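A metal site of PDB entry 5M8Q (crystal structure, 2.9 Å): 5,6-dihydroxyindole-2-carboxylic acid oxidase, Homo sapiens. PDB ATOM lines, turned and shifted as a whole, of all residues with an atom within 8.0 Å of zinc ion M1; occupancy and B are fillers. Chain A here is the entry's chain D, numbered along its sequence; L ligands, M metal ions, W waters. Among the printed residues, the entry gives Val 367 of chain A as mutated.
A ring nitrogen (ND1) of His 353 lies within hydrogen-bond range of the side-chain amide oxygen (OD1) of Asn 354 (3.0 Å). ND1 of His 353 is in hydrogen-bond range of O of Glu 336 (2.9 Å). The backbone carbonyl oxygen (O) of Gly 364 sits at hydrogen-bond distance from a ring nitrogen (ND1) of His 357 (2.8 Å).
Water W1 binds zinc ion M1 (1.9 Å). A ring nitrogen (NE2) of His 380 binds zinc ion M1 (1.9 Å). NE2 of His 353 is bound to zinc ion M1, at 2.0 Å. NE2 of His 357 binds zinc ion M1 (2.1 Å). Zinc ion M1 has four donor atoms within binding distance.
O2 of the ligand sits close to NE2 of His 353, at 3.5 Å. A ring nitrogen (NE2) of His 191 lies close to an oxygen (O2) of the ligand (3.3 Å). An oxygen (O1) of the ligand lies within hydrogen-bond range of the side-chain hydroxyl (OG) of Ser 370 (2.9 Å).
CE2 of Phe 376 touches zinc ion M1, 3.8 Å away. Four residues have an atom within 4 Å of zinc ion M1: His 353, His 357, Phe 376 and His 380. The nearest printed residue that does not touch zinc ion M1 is His 200 (4.3 Å).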
ATOM      1  N   HIS A 168      12.676  -6.350 -16.126  1.00  0.00           N
ATOM      2  CA  HIS A 168      13.066  -7.446 -15.248  1.00  0.00           C
ATOM      3  C   HIS A 168      12.244  -7.444 -13.959  1.00  0.00           C
ATOM      4  O   HIS A 168      11.878  -8.513 -13.456  1.00  0.00           O
ATOM      5  CB  HIS A 168      14.555  -7.350 -14.955  1.00  0.00           C
ATOM      6  CG  HIS A 168      15.093  -8.447 -14.102  1.00  0.00           C
ATOM      7  ND1 HIS A 168      15.051  -8.409 -12.724  1.00  0.00           N
ATOM      8  CD2 HIS A 168      15.743  -9.593 -14.423  1.00  0.00           C
ATOM      9  CE1 HIS A 168      15.632  -9.497 -12.238  1.00  0.00           C
ATOM     10  NE2 HIS A 168      16.061 -10.228 -13.253  1.00  0.00           N
ATOM     11  N   SER A 190      10.591 -15.131 -15.422  1.00  0.00           N
ATOM     12  CA  SER A 190      11.921 -15.043 -15.988  1.00  0.00           C
ATOM     13  C   SER A 190      12.967 -15.831 -15.220  1.00  0.00           C
ATOM     14  O   SER A 190      14.130 -15.850 -15.642  1.00  0.00           O
ATOM     15  CB  SER A 190      12.353 -13.573 -16.050  1.00  0.00           C
ATOM     16  OG  SER A 190      12.103 -12.948 -14.778  1.00  0.00           O
ATOM     17  N   HIS A 191      12.602 -16.454 -14.087  1.00  0.00           N
ATOM     18  CA  HIS A 191      13.503 -17.241 -13.258  1.00  0.00           C
ATOM     19  C   HIS A 191      12.807 -18.519 -12.832  1.00  0.00           C
ATOM     20  O   HIS A 191      11.581 -18.660 -12.965  1.00  0.00           O
ATOM     21  CB  HIS A 191      13.916 -16.533 -11.972  1.00  0.00           C
ATOM     22  CG  HIS A 191      14.419 -15.159 -12.204  1.00  0.00           C
ATOM     23  ND1 HIS A 191      13.566 -14.081 -12.386  1.00  0.00           N
ATOM     24  CD2 HIS A 191      15.672 -14.677 -12.297  1.00  0.00           C
ATOM     25  CE1 HIS A 191      14.300 -12.994 -12.591  1.00  0.00           C
ATOM     26  NE2 HIS A 191      15.581 -13.329 -12.513  1.00  0.00           N
ATOM     27  N   PHE A 196      14.389 -18.877 -18.258  1.00  0.00           N
ATOM     28  CA  PHE A 196      15.349 -17.989 -17.618  1.00  0.00           C
ATOM     29  C   PHE A 196      16.433 -17.528 -18.598  1.00  0.00           C
ATOM     30  O   PHE A 196      16.677 -16.325 -18.726  1.00  0.00           O
ATOM     31  CB  PHE A 196      15.950 -18.695 -16.404  1.00  0.00           C
ATOM     32  CG  PHE A 196      17.272 -18.160 -15.998  1.00  0.00           C
ATOM     33  CD1 PHE A 196      17.362 -16.941 -15.355  1.00  0.00           C
ATOM     34  CD2 PHE A 196      18.431 -18.859 -16.278  1.00  0.00           C
ATOM     35  CE1 PHE A 196      18.599 -16.427 -14.974  1.00  0.00           C
ATOM     36  CE2 PHE A 196      19.661 -18.366 -15.902  1.00  0.00           C
ATOM     37  CZ  PHE A 196      19.752 -17.147 -15.241  1.00  0.00           C
ATOM     38  N   HIS A 200      16.558 -13.702 -20.438  1.00  0.00           N
ATOM     39  CA  HIS A 200      17.692 -12.811 -20.241  1.00  0.00           C
ATOM     40  C   HIS A 200      18.497 -12.619 -21.531  1.00  0.00           C
ATOM     41  O   HIS A 200      19.006 -11.524 -21.794  1.00  0.00           O
ATOM     42  CB  HIS A 200      18.547 -13.331 -19.090  1.00  0.00           C
ATOM     43  CG  HIS A 200      17.886 -13.145 -17.755  1.00  0.00           C
ATOM     44  ND1 HIS A 200      16.877 -13.965 -17.306  1.00  0.00           N
ATOM     45  CD2 HIS A 200      18.063 -12.199 -16.800  1.00  0.00           C
ATOM     46  CE1 HIS A 200      16.470 -13.539 -16.121  1.00  0.00           C
ATOM     47  NE2 HIS A 200      17.174 -12.466 -15.782  1.00  0.00           N
ATOM     48  N   HIS A 203      16.555  -9.992 -23.068  1.00  0.00           N
ATOM     49  CA  HIS A 203      16.811  -8.835 -22.207  1.00  0.00           C
ATOM     50  C   HIS A 203      18.094  -8.121 -22.635  1.00  0.00           C
ATOM     51  O   HIS A 203      18.139  -6.891 -22.776  1.00  0.00           O
ATOM     52  CB  HIS A 203      16.887  -9.327 -20.765  1.00  0.00           C
ATOM     53  CG  HIS A 203      16.766  -8.257 -19.720  1.00  0.00           C
ATOM     54  ND1 HIS A 203      17.403  -8.334 -18.505  1.00  0.00           N
ATOM     55  CD2 HIS A 203      16.038  -7.116 -19.690  1.00  0.00           C
ATOM     56  CE1 HIS A 203      17.090  -7.278 -17.780  1.00  0.00           C
ATOM     57  NE2 HIS A 203      16.263  -6.518 -18.479  1.00  0.00           N
ATOM     58  N   GLU A 336      21.518 -21.499 -14.123  1.00  0.00           N
ATOM     59  CA  GLU A 336      20.802 -20.550 -13.275  1.00  0.00           C
ATOM     60  C   GLU A 336      21.297 -20.643 -11.850  1.00  0.00           C
ATOM     61  O   GLU A 336      21.508 -19.621 -11.187  1.00  0.00           O
ATOM     62  CB  GLU A 336      19.299 -20.775 -13.357  1.00  0.00           C
ATOM     63  CG  GLU A 336      18.521 -19.700 -12.606  1.00  0.00           C
ATOM     64  CD  GLU A 336      17.021 -19.780 -12.834  1.00  0.00           C
ATOM     65  OE1 GLU A 336      16.585 -20.444 -13.801  1.00  0.00           O
ATOM     66  OE2 GLU A 336      16.271 -19.176 -12.043  1.00  0.00           O
ATOM     67  N   HIS A 353      25.166 -18.698 -11.870  1.00  0.00           N
ATOM     68  CA  HIS A 353      24.509 -17.390 -11.985  1.00  0.00           C
ATOM     69  C   HIS A 353      23.965 -16.910 -10.643  1.00  0.00           C
ATOM     70  O   HIS A 353      24.149 -15.749 -10.276  1.00  0.00           O
ATOM     71  CB  HIS A 353      23.412 -17.441 -13.034  1.00  0.00           C
ATOM     72  CG  HIS A 353      22.285 -16.490 -12.800  1.00  0.00           C
ATOM     73  ND1 HIS A 353      21.155 -16.830 -12.073  1.00  0.00           N
ATOM     74  CD2 HIS A 353      22.071 -15.225 -13.239  1.00  0.00           C
ATOM     75  CE1 HIS A 353      20.316 -15.806 -12.052  1.00  0.00           C
ATOM     76  NE2 HIS A 353      20.848 -14.821 -12.755  1.00  0.00           N
ATOM     77  N   ASN A 354      23.319 -17.790  -9.890  1.00  0.00           N
ATOM     78  CA  ASN A 354      22.838 -17.403  -8.567  1.00  0.00           C
ATOM     79  C   ASN A 354      23.992 -17.012  -7.659  1.00  0.00           C
ATOM     80  O   ASN A 354      23.958 -15.979  -6.983  1.00  0.00           O
ATOM     81  CB  ASN A 354      22.021 -18.523  -7.946  1.00  0.00           C
ATOM     82  CG  ASN A 354      20.645 -18.637  -8.545  1.00  0.00           C
ATOM     83  OD1 ASN A 354      20.265 -17.840  -9.414  1.00  0.00           O
ATOM     84  ND2 ASN A 354      19.880 -19.616  -8.073  1.00  0.00           N
ATOM     85  N   ALA A 356      26.908 -15.800  -8.317  1.00  0.00           N
ATOM     86  CA  ALA A 356      27.462 -14.483  -8.637  1.00  0.00           C
ATOM     87  C   ALA A 356      26.552 -13.371  -8.122  1.00  0.00           C
ATOM     88  O   ALA A 356      27.046 -12.346  -7.620  1.00  0.00           O
ATOM     89  CB  ALA A 356      27.676 -14.371 -10.142  1.00  0.00           C
ATOM     90  N   HIS A 357      25.234 -13.545  -8.220  1.00  0.00           N
ATOM     91  CA  HIS A 357      24.308 -12.525  -7.744  1.00  0.00           C
ATOM     92  C   HIS A 357      24.458 -12.291  -6.252  1.00  0.00           C
ATOM     93  O   HIS A 357      24.648 -11.164  -5.792  1.00  0.00           O
ATOM     94  CB  HIS A 357      22.884 -12.941  -8.070  1.00  0.00           C
ATOM     95  CG  HIS A 357      22.363 -12.444  -9.378  1.00  0.00           C
ATOM     96  ND1 HIS A 357      22.023 -11.126  -9.580  1.00  0.00           N
ATOM     97  CD2 HIS A 357      22.107 -13.087 -10.540  1.00  0.00           C
ATOM     98  CE1 HIS A 357      21.569 -10.976 -10.817  1.00  0.00           C
ATOM     99  NE2 HIS A 357      21.621 -12.159 -11.417  1.00  0.00           N
ATOM    100  N   GLY A 364      22.555  -5.899  -6.309  1.00  0.00           N
ATOM    101  CA  GLY A 364      22.593  -6.981  -7.280  1.00  0.00           C
ATOM    102  C   GLY A 364      22.176  -8.329  -6.735  1.00  0.00           C
ATOM    103  O   GLY A 364      21.981  -9.248  -7.538  1.00  0.00           O
ATOM    104  N   VAL A 367      16.246  -9.889  -6.120  1.00  0.00           N
ATOM    105  CA  VAL A 367      15.564 -10.270  -7.355  1.00  0.00           C
ATOM    106  C   VAL A 367      14.862  -9.088  -8.009  1.00  0.00           C
ATOM    107  O   VAL A 367      14.939  -8.892  -9.230  1.00  0.00           O
ATOM    108  CB  VAL A 367      14.607 -11.432  -7.049  1.00  0.00           C
ATOM    109  CG1 VAL A 367      15.335 -12.413  -6.151  1.00  0.00           C
ATOM    110  CG2 VAL A 367      13.369 -10.944  -6.322  1.00  0.00           C
ATOM    111  N   SER A 370      17.910  -6.140  -8.998  1.00  0.00           N
ATOM    112  CA  SER A 370      19.321  -6.368  -9.305  1.00  0.00           C
ATOM    113  C   SER A 370      19.825  -5.676 -10.579  1.00  0.00           C
ATOM    114  O   SER A 370      20.965  -5.187 -10.557  1.00  0.00           O
ATOM    115  CB  SER A 370      19.621  -7.870  -9.335  1.00  0.00           C
ATOM    116  OG  SER A 370      18.929  -8.545 -10.363  1.00  0.00           O
ATOM    117  N   PRO A 371      19.065  -5.570 -11.678  1.00  0.00           N
ATOM    118  CA  PRO A 371      19.654  -4.899 -12.859  1.00  0.00           C
ATOM    119  C   PRO A 371      20.049  -3.441 -12.577  1.00  0.00           C
ATOM    120  O   PRO A 371      20.668  -2.774 -13.430  1.00  0.00           O
ATOM    121  CB  PRO A 371      18.548  -4.999 -13.913  1.00  0.00           C
ATOM    122  CG  PRO A 371      17.596  -6.044 -13.406  1.00  0.00           C
ATOM    123  CD  PRO A 371      17.683  -6.017 -11.931  1.00  0.00           C
ATOM    124  N   PHE A 376      25.214  -6.351 -13.464  1.00  0.00           N
ATOM    125  CA  PHE A 376      24.211  -7.282 -13.975  1.00  0.00           C
ATOM    126  C   PHE A 376      24.424  -7.546 -15.475  1.00  0.00           C
ATOM    127  O   PHE A 376      24.491  -8.706 -15.914  1.00  0.00           O
ATOM    128  CB  PHE A 376      22.815  -6.730 -13.714  1.00  0.00           C
ATOM    129  CG  PHE A 376      21.705  -7.593 -14.208  1.00  0.00           C
ATOM    130  CD1 PHE A 376      21.284  -7.526 -15.521  1.00  0.00           C
ATOM    131  CD2 PHE A 376      21.040  -8.447 -13.338  1.00  0.00           C
ATOM    132  CE1 PHE A 376      20.229  -8.316 -15.973  1.00  0.00           C
ATOM    133  CE2 PHE A 376      19.995  -9.224 -13.779  1.00  0.00           C
ATOM    134  CZ  PHE A 376      19.581  -9.158 -15.098  1.00  0.00           C
ATOM    135  N   LEU A 379      27.141  -9.777 -15.860  1.00  0.00           N
ATOM    136  CA  LEU A 379      26.817 -11.062 -15.241  1.00  0.00           C
ATOM    137  C   LEU A 379      25.972 -11.904 -16.195  1.00  0.00           C
ATOM    138  O   LEU A 379      26.119 -13.122 -16.250  1.00  0.00           O
ATOM    139  CB  LEU A 379      26.072 -10.847 -13.919  1.00  0.00           C
ATOM    140  CG  LEU A 379      26.125 -11.984 -12.894  1.00  0.00           C
ATOM    141  CD1 LEU A 379      25.718 -11.511 -11.508  1.00  0.00           C
ATOM    142  CD2 LEU A 379      25.286 -13.165 -13.323  1.00  0.00           C
ATOM    143  N   HIS A 380      25.108 -11.263 -16.971  1.00  0.00           N
ATOM    144  CA  HIS A 380      24.208 -12.033 -17.795  1.00  0.00           C
ATOM    145  C   HIS A 380      24.695 -12.224 -19.219  1.00  0.00           C
ATOM    146  O   HIS A 380      24.239 -13.164 -19.881  1.00  0.00           O
ATOM    147  CB  HIS A 380      22.818 -11.422 -17.762  1.00  0.00           C
ATOM    148  CG  HIS A 380      21.983 -11.991 -16.678  1.00  0.00           C
ATOM    149  ND1 HIS A 380      21.232 -13.141 -16.841  1.00  0.00           N
ATOM    150  CD2 HIS A 380      21.839 -11.632 -15.380  1.00  0.00           C
ATOM    151  CE1 HIS A 380      20.646 -13.443 -15.694  1.00  0.00           C
ATOM    152  NE2 HIS A 380      21.001 -12.538 -14.801  1.00  0.00           N
ATOM    153  N   THR A 383      26.590 -15.432 -18.528  1.00  0.00           N
ATOM    154  CA  THR A 383      25.588 -16.494 -18.470  1.00  0.00           C
ATOM    155  C   THR A 383      25.010 -16.761 -19.834  1.00  0.00           C
ATOM    156  O   THR A 383      24.706 -17.895 -20.195  1.00  0.00           O
ATOM    157  CB  THR A 383      24.464 -16.127 -17.517  1.00  0.00           C
ATOM    158  OG1 THR A 383      25.016 -15.648 -16.281  1.00  0.00           O
ATOM    159  CG2 THR A 383      23.610 -17.314 -17.222  1.00  0.00           C
HETATM  160  C1  LIG L   1      18.872 -11.490  -8.180  1.00  0.00           C
HETATM  161  C2  LIG L   1      18.441 -12.001  -9.323  1.00  0.00           C
HETATM  162  C3  LIG L   1      18.634 -13.419  -9.598  1.00  0.00           C
HETATM  163  C4  LIG L   1      19.274 -14.311  -8.615  1.00  0.00           C
HETATM  164  C5  LIG L   1      19.693 -13.827  -7.465  1.00  0.00           C
HETATM  165  C6  LIG L   1      20.348 -14.748  -6.442  1.00  0.00           C
HETATM  166  O1  LIG L   1      17.803 -11.238 -10.334  1.00  0.00           O
HETATM  167  O2  LIG L   1      18.251 -13.834 -10.647  1.00  0.00           O
HETATM  168  O3  LIG L   1      19.511 -12.382  -7.197  1.00  0.00           O
HETATM  169  O4  LIG L   1      19.719 -14.525  -5.202  1.00  0.00           O
HETATM  170 ZN    ZN M   1      20.458 -12.895 -12.979  1.00  0.00          ZN
HETATM  171 ZN    ZN M   2      17.129 -12.104 -13.118  1.00  0.00          ZN
HETATM  172  O   HOH W   1      19.011 -11.806 -12.394  1.00  0.00           O
